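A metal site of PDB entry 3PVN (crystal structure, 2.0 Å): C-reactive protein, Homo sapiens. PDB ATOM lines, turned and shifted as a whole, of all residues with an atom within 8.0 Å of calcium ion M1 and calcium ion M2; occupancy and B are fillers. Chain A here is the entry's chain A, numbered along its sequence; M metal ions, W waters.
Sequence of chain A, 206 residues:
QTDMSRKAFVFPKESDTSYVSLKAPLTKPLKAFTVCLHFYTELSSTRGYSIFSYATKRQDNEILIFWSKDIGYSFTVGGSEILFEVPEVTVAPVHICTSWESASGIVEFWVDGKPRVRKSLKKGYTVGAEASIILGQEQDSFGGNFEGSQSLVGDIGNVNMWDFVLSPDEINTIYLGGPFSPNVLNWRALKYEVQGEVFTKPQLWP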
ATOM      1  N   SER A  50     -18.471 -16.988  27.951  1.00  0.00           N
ATOM      2  CA  SER A  50     -17.947 -15.651  28.049  1.00  0.00           C
ATOM      3  C   SER A  50     -18.995 -14.604  27.584  1.00  0.00           C
ATOM      4  O   SER A  50     -19.682 -14.786  26.536  1.00  0.00           O
ATOM      5  CB  SER A  50     -16.700 -15.558  27.201  1.00  0.00           C
ATOM      6  OG  SER A  50     -16.171 -14.256  27.237  1.00  0.00           O
ATOM      7  N   SER A  53     -15.058 -10.099  26.642  1.00  0.00           N
ATOM      8  CA  SER A  53     -13.643 -10.550  26.774  1.00  0.00           C
ATOM      9  C   SER A  53     -12.652  -9.507  26.255  1.00  0.00           C
ATOM     10  O   SER A  53     -12.604  -9.168  25.081  1.00  0.00           O
ATOM     11  CB  SER A  53     -13.467 -11.876  26.057  1.00  0.00           C
ATOM     12  OG  SER A  53     -12.082 -12.293  26.079  1.00  0.00           O
ATOM     13  N   TYR A  54     -11.882  -8.982  27.150  1.00  0.00           N
ATOM     14  CA  TYR A  54     -10.939  -7.879  26.855  1.00  0.00           C
ATOM     15  C   TYR A  54      -9.527  -8.409  27.246  1.00  0.00           C
ATOM     16  O   TYR A  54      -9.277  -8.777  28.399  1.00  0.00           O
ATOM     17  CB  TYR A  54     -11.376  -6.664  27.694  1.00  0.00           C
ATOM     18  CG  TYR A  54     -10.656  -5.330  27.612  1.00  0.00           C
ATOM     19  CD1 TYR A  54      -9.369  -5.161  28.131  1.00  0.00           C
ATOM     20  CD2 TYR A  54     -11.324  -4.199  27.120  1.00  0.00           C
ATOM     21  CE1 TYR A  54      -8.731  -3.949  28.061  1.00  0.00           C
ATOM     22  CE2 TYR A  54     -10.702  -2.951  27.062  1.00  0.00           C
ATOM     23  CZ  TYR A  54      -9.403  -2.845  27.515  1.00  0.00           C
ATOM     24  OH  TYR A  54      -8.824  -1.617  27.476  1.00  0.00           O
ATOM     25  N   ALA A  55      -8.653  -8.480  26.258  1.00  0.00           N
ATOM     26  CA  ALA A  55      -7.328  -9.031  26.461  1.00  0.00           C
ATOM     27  C   ALA A  55      -6.239  -8.048  26.040  1.00  0.00           C
ATOM     28  O   ALA A  55      -6.432  -7.271  25.102  1.00  0.00           O
ATOM     29  CB  ALA A  55      -7.163 -10.358  25.659  1.00  0.00           C
ATOM     30  N   GLN A  59      -1.982 -10.128  29.009  1.00  0.00           N
ATOM     31  CA  GLN A  59      -2.976 -10.711  29.936  1.00  0.00           C
ATOM     32  C   GLN A  59      -4.282 -11.000  29.157  1.00  0.00           C
ATOM     33  O   GLN A  59      -4.910 -10.063  28.644  1.00  0.00           O
ATOM     34  CB  GLN A  59      -3.230  -9.755  31.151  1.00  0.00           C
ATOM     35  CG  GLN A  59      -4.412 -10.198  32.041  1.00  0.00           C
ATOM     36  CD  GLN A  59      -4.183 -11.530  32.716  1.00  0.00           C
ATOM     37  OE1 GLN A  59      -4.821 -12.557  32.384  1.00  0.00           O
ATOM     38  NE2 GLN A  59      -3.306 -11.529  33.679  1.00  0.00           N
ATOM     39  N   ASP A  60      -4.622 -12.296  28.984  1.00  0.00           N
ATOM     40  CA  ASP A  60      -5.789 -12.694  28.160  1.00  0.00           C
ATOM     41  C   ASP A  60      -7.095 -12.252  28.826  1.00  0.00           C
ATOM     42  O   ASP A  60      -8.049 -11.896  28.142  1.00  0.00           O
ATOM     43  CB  ASP A  60      -5.826 -14.234  27.850  1.00  0.00           C
ATOM     44  CG  ASP A  60      -5.614 -15.074  29.073  1.00  0.00           C
ATOM     45  OD1 ASP A  60      -4.759 -14.677  29.892  1.00  0.00           O
ATOM     46  OD2 ASP A  60      -6.301 -16.108  29.240  1.00  0.00           O
ATOM     47  N   ASN A  61      -7.102 -12.321  30.145  1.00  0.00           N
ATOM     48  CA  ASN A  61      -8.236 -11.908  30.991  1.00  0.00           C
ATOM     49  C   ASN A  61      -8.039 -10.561  31.679  1.00  0.00           C
ATOM     50  O   ASN A  61      -8.115 -10.506  32.887  1.00  0.00           O
ATOM     51  CB  ASN A  61      -8.478 -13.016  32.008  1.00  0.00           C
ATOM     52  CG  ASN A  61      -8.838 -14.390  31.332  1.00  0.00           C
ATOM     53  OD1 ASN A  61      -9.116 -14.472  30.131  1.00  0.00           O
ATOM     54  ND2 ASN A  61      -8.878 -15.441  32.149  1.00  0.00           N
ATOM     55  N   GLU A  62      -7.746  -9.510  30.925  1.00  0.00           N
ATOM     56  CA  GLU A  62      -7.510  -8.146  31.458  1.00  0.00           C
ATOM     57  C   GLU A  62      -8.859  -7.593  31.983  1.00  0.00           C
ATOM     58  O   GLU A  62      -8.876  -6.944  33.053  1.00  0.00           O
ATOM     59  CB  GLU A  62      -6.938  -7.240  30.395  1.00  0.00           C
ATOM     60  CG  GLU A  62      -6.586  -5.809  30.879  1.00  0.00           C
ATOM     61  CD  GLU A  62      -5.309  -5.719  31.773  1.00  0.00           C
ATOM     62  OE1 GLU A  62      -4.981  -6.692  32.519  1.00  0.00           O
ATOM     63  OE2 GLU A  62      -4.636  -4.648  31.704  1.00  0.00           O
ATOM     64  N   LEU A  64     -12.838  -9.629  32.145  1.00  0.00           N
ATOM     65  CA  LEU A  64     -13.631 -10.753  31.651  1.00  0.00           C
ATOM     66  C   LEU A  64     -14.922 -10.877  32.452  1.00  0.00           C
ATOM     67  O   LEU A  64     -14.881 -11.036  33.657  1.00  0.00           O
ATOM     68  CB  LEU A  64     -12.823 -12.087  31.741  1.00  0.00           C
ATOM     69  CG  LEU A  64     -13.600 -13.393  31.407  1.00  0.00           C
ATOM     70  CD1 LEU A  64     -14.103 -13.362  29.980  1.00  0.00           C
ATOM     71  CD2 LEU A  64     -12.692 -14.641  31.523  1.00  0.00           C
ATOM     72  N   PHE A  66     -18.127 -13.323  32.742  1.00  0.00           N
ATOM     73  CA  PHE A  66     -18.279 -14.700  32.385  1.00  0.00           C
ATOM     74  C   PHE A  66     -19.394 -15.254  33.202  1.00  0.00           C
ATOM     75  O   PHE A  66     -19.603 -14.818  34.351  1.00  0.00           O
ATOM     76  CB  PHE A  66     -16.932 -15.436  32.662  1.00  0.00           C
ATOM     77  CG  PHE A  66     -16.832 -16.862  32.103  1.00  0.00           C
ATOM     78  CD1 PHE A  66     -16.281 -17.079  30.818  1.00  0.00           C
ATOM     79  CD2 PHE A  66     -17.263 -17.985  32.863  1.00  0.00           C
ATOM     80  CE1 PHE A  66     -16.184 -18.342  30.275  1.00  0.00           C
ATOM     81  CE2 PHE A  66     -17.144 -19.322  32.323  1.00  0.00           C
ATOM     82  CZ  PHE A  66     -16.609 -19.497  31.009  1.00  0.00           C
ATOM     83  N   GLN A 137     -16.851 -15.006  22.139  1.00  0.00           N
ATOM     84  CA  GLN A 137     -15.824 -16.035  22.492  1.00  0.00           C
ATOM     85  C   GLN A 137     -14.949 -15.520  23.635  1.00  0.00           C
ATOM     86  O   GLN A 137     -14.808 -14.308  23.840  1.00  0.00           O
ATOM     87  CB  GLN A 137     -14.894 -16.399  21.304  1.00  0.00           C
ATOM     88  CG  GLN A 137     -15.500 -16.900  20.011  1.00  0.00           C
ATOM     89  CD  GLN A 137     -16.146 -18.288  20.063  1.00  0.00           C
ATOM     90  OE1 GLN A 137     -17.101 -18.592  19.272  1.00  0.00           O
ATOM     91  NE2 GLN A 137     -15.689 -19.123  20.956  1.00  0.00           N
ATOM     92  N   GLU A 138     -14.348 -16.473  24.338  1.00  0.00           N
ATOM     93  CA  GLU A 138     -13.458 -16.184  25.435  1.00  0.00           C
ATOM     94  C   GLU A 138     -12.023 -16.297  24.936  1.00  0.00           C
ATOM     95  O   GLU A 138     -11.604 -17.394  24.499  1.00  0.00           O
ATOM     96  CB  GLU A 138     -13.706 -17.176  26.555  1.00  0.00           C
ATOM     97  CG  GLU A 138     -13.287 -16.641  27.904  1.00  0.00           C
ATOM     98  CD  GLU A 138     -11.730 -16.505  28.046  1.00  0.00           C
ATOM     99  OE1 GLU A 138     -11.005 -17.533  27.952  1.00  0.00           O
ATOM    100  OE2 GLU A 138     -11.262 -15.335  28.249  1.00  0.00           O
ATOM    101  N   GLN A 139     -11.273 -15.193  24.985  1.00  0.00           N
ATOM    102  CA  GLN A 139      -9.812 -15.173  24.596  1.00  0.00           C
ATOM    103  C   GLN A 139      -8.852 -15.825  25.539  1.00  0.00           C
ATOM    104  O   GLN A 139      -8.822 -15.514  26.732  1.00  0.00           O
ATOM    105  CB  GLN A 139      -9.316 -13.746  24.379  1.00  0.00           C
ATOM    106  CG  GLN A 139     -10.013 -13.038  23.242  1.00  0.00           C
ATOM    107  CD  GLN A 139      -9.770 -11.587  23.309  1.00  0.00           C
ATOM    108  OE1 GLN A 139     -10.335 -10.845  24.189  1.00  0.00           O
ATOM    109  NE2 GLN A 139      -8.886 -11.113  22.425  1.00  0.00           N
ATOM    110  N   ASP A 140      -8.003 -16.722  24.983  1.00  0.00           N
ATOM    111  CA  ASP A 140      -6.854 -17.239  25.693  1.00  0.00           C
ATOM    112  C   ASP A 140      -5.547 -16.641  25.138  1.00  0.00           C
ATOM    113  O   ASP A 140      -4.491 -16.860  25.683  1.00  0.00           O
ATOM    114  CB  ASP A 140      -6.843 -18.779  25.705  1.00  0.00           C
ATOM    115  CG  ASP A 140      -7.734 -19.364  26.773  1.00  0.00           C
ATOM    116  OD1 ASP A 140      -8.111 -18.661  27.739  1.00  0.00           O
ATOM    117  OD2 ASP A 140      -8.131 -20.549  26.673  1.00  0.00           O
ATOM    118  N   SER A 141      -5.622 -15.867  24.076  1.00  0.00           N
ATOM    119  CA  SER A 141      -4.473 -15.066  23.622  1.00  0.00           C
ATOM    120  C   SER A 141      -5.027 -13.783  23.044  1.00  0.00           C
ATOM    121  O   SER A 141      -6.254 -13.662  22.914  1.00  0.00           O
ATOM    122  CB  SER A 141      -3.651 -15.819  22.573  1.00  0.00           C
ATOM    123  OG  SER A 141      -4.364 -15.912  21.324  1.00  0.00           O
ATOM    124  N   GLY A 144      -7.396 -14.227  20.031  1.00  0.00           N
ATOM    125  CA  GLY A 144      -7.511 -15.606  19.559  1.00  0.00           C
ATOM    126  C   GLY A 144      -7.569 -16.686  20.600  1.00  0.00           C
ATOM    127  O   GLY A 144      -7.931 -16.454  21.729  1.00  0.00           O
ATOM    128  N   ASN A 145      -7.222 -17.894  20.191  1.00  0.00           N
ATOM    129  CA  ASN A 145      -7.305 -19.073  21.033  1.00  0.00           C
ATOM    130  C   ASN A 145      -8.656 -19.264  21.739  1.00  0.00           C
ATOM    131  O   ASN A 145      -8.724 -19.328  22.973  1.00  0.00           O
ATOM    132  CB  ASN A 145      -6.116 -19.171  22.001  1.00  0.00           C
ATOM    133  CG  ASN A 145      -4.852 -19.728  21.312  1.00  0.00           C
ATOM    134  OD1 ASN A 145      -4.095 -18.986  20.717  1.00  0.00           O
ATOM    135  ND2 ASN A 145      -4.678 -21.053  21.359  1.00  0.00           N
ATOM    136  N   PHE A 146      -9.711 -19.372  20.962  1.00  0.00           N
ATOM    137  CA  PHE A 146     -11.071 -19.515  21.496  1.00  0.00           C
ATOM    138  C   PHE A 146     -11.416 -20.984  21.892  1.00  0.00           C
ATOM    139  O   PHE A 146     -10.883 -21.917  21.320  1.00  0.00           O
ATOM    140  CB  PHE A 146     -12.084 -18.969  20.475  1.00  0.00           C
ATOM    141  CG  PHE A 146     -11.723 -17.605  19.943  1.00  0.00           C
ATOM    142  CD1 PHE A 146     -11.364 -16.582  20.819  1.00  0.00           C
ATOM    143  CD2 PHE A 146     -11.737 -17.333  18.574  1.00  0.00           C
ATOM    144  CE1 PHE A 146     -11.031 -15.301  20.340  1.00  0.00           C
ATOM    145  CE2 PHE A 146     -11.435 -16.061  18.080  1.00  0.00           C
ATOM    146  CZ  PHE A 146     -11.045 -15.037  18.977  1.00  0.00           C
ATOM    147  N   GLU A 147     -12.288 -21.179  22.879  1.00  0.00           N
ATOM    148  CA  GLU A 147     -12.801 -22.508  23.224  1.00  0.00           C
ATOM    149  C   GLU A 147     -14.285 -22.507  22.973  1.00  0.00           C
ATOM    150  O   GLU A 147     -15.009 -21.666  23.520  1.00  0.00           O
ATOM    151  CB  GLU A 147     -12.533 -22.871  24.685  1.00  0.00           C
ATOM    152  CG  GLU A 147     -11.034 -23.032  24.992  1.00  0.00           C
ATOM    153  CD  GLU A 147     -10.719 -23.429  26.461  1.00  0.00           C
ATOM    154  OE1 GLU A 147     -10.707 -22.554  27.384  1.00  0.00           O
ATOM    155  OE2 GLU A 147     -10.377 -24.630  26.675  1.00  0.00           O
ATOM    156  N   GLY A 148     -14.754 -23.437  22.125  1.00  0.00           N
ATOM    157  CA  GLY A 148     -16.193 -23.583  21.867  1.00  0.00           C
ATOM    158  C   GLY A 148     -17.038 -23.857  23.086  1.00  0.00           C
ATOM    159  O   GLY A 148     -18.232 -23.545  23.111  1.00  0.00           O
ATOM    160  N   SER A 149     -16.444 -24.466  24.109  1.00  0.00           N
ATOM    161  CA  SER A 149     -17.163 -24.791  25.340  1.00  0.00           C
ATOM    162  C   SER A 149     -17.421 -23.508  26.223  1.00  0.00           C
ATOM    163  O   SER A 149     -18.081 -23.603  27.251  1.00  0.00           O
ATOM    164  CB  SER A 149     -16.388 -25.834  26.143  1.00  0.00           C
ATOM    165  OG  SER A 149     -15.163 -25.294  26.680  1.00  0.00           O
ATOM    166  N   GLN A 150     -16.879 -22.366  25.801  1.00  0.00           N
ATOM    167  CA  GLN A 150     -17.110 -21.062  26.465  1.00  0.00           C
ATOM    168  C   GLN A 150     -17.710 -20.030  25.452  1.00  0.00           C
ATOM    169  O   GLN A 150     -17.770 -18.835  25.728  1.00  0.00           O
ATOM    170  CB  GLN A 150     -15.792 -20.510  27.046  1.00  0.00           C
ATOM    171  CG  GLN A 150     -15.051 -21.444  28.071  1.00  0.00           C
ATOM    172  CD  GLN A 150     -13.631 -20.931  28.446  1.00  0.00           C
ATOM    173  OE1 GLN A 150     -12.945 -20.344  27.623  1.00  0.00           O
ATOM    174  NE2 GLN A 150     -13.221 -21.144  29.705  1.00  0.00           N
HETATM  175 CA    CA M   1     -10.541 -19.935  27.524  1.00  0.00          CA
HETATM  176 CA    CA M   2      -8.959 -16.627  28.833  1.00  0.00          CA
HETATM  177  O   HOH W   1     -10.745 -19.569  24.913  1.00  0.00           O
HETATM  178  O   HOH W   2      -9.702 -19.088  30.828  1.00  0.00           O
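OG of Ser 53 sits at hydrogen-bond distance from OE1 of Gln 139, 3.0 Å away. N of Ser 50 is in hydrogen-bond range of O of Gln 150, at 3.0 Å. The backbone carbonyl oxygen of Asn 145 sits close to the backbone NH of Asp 140 (3.4 Å). The side-chain amide oxygen (OE1) of Gln 59 is in hydrogen-bond range of the backbone NH (N) of Asn 61. The side-chain amide oxygen (OE1) of Gln 59 sits close to the side-chain carboxylate (OD1) of Asp 60, 3.3 Å away.
Calcium ion M2 is bound by O of Gln 139 (2.4 Å), OE1 of Glu 138 (2.4 Å), OD1 of Asp 140 (2.5 Å), OD1 of Asn 61 (2.5 Å), OE2 of Glu 138 (2.7 Å) and OD2 of Asp 60 (2.7 Å).
Within 4 Å of calcium ion M2: Asp 60, Asn 61, Glu 138, Gln 139 and Asp 140. The nearest printed residue that does not touch calcium ion M2 is Leu 64 (5.0 Å).
The nearest printed residue that does not touch calcium ion M1 is Gln 139 (4.8 Å).
Calcium ion M1 is bound by OE1 of Gln 150 (2.4 Å), OE1 of Glu 138 (2.5 Å), OE1 of Glu 147 (2.6 Å), OD2 of Asp 140 (2.6 Å), water W1 (2.6 Å) and OD1 of Asp 140 (2.8 Å).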
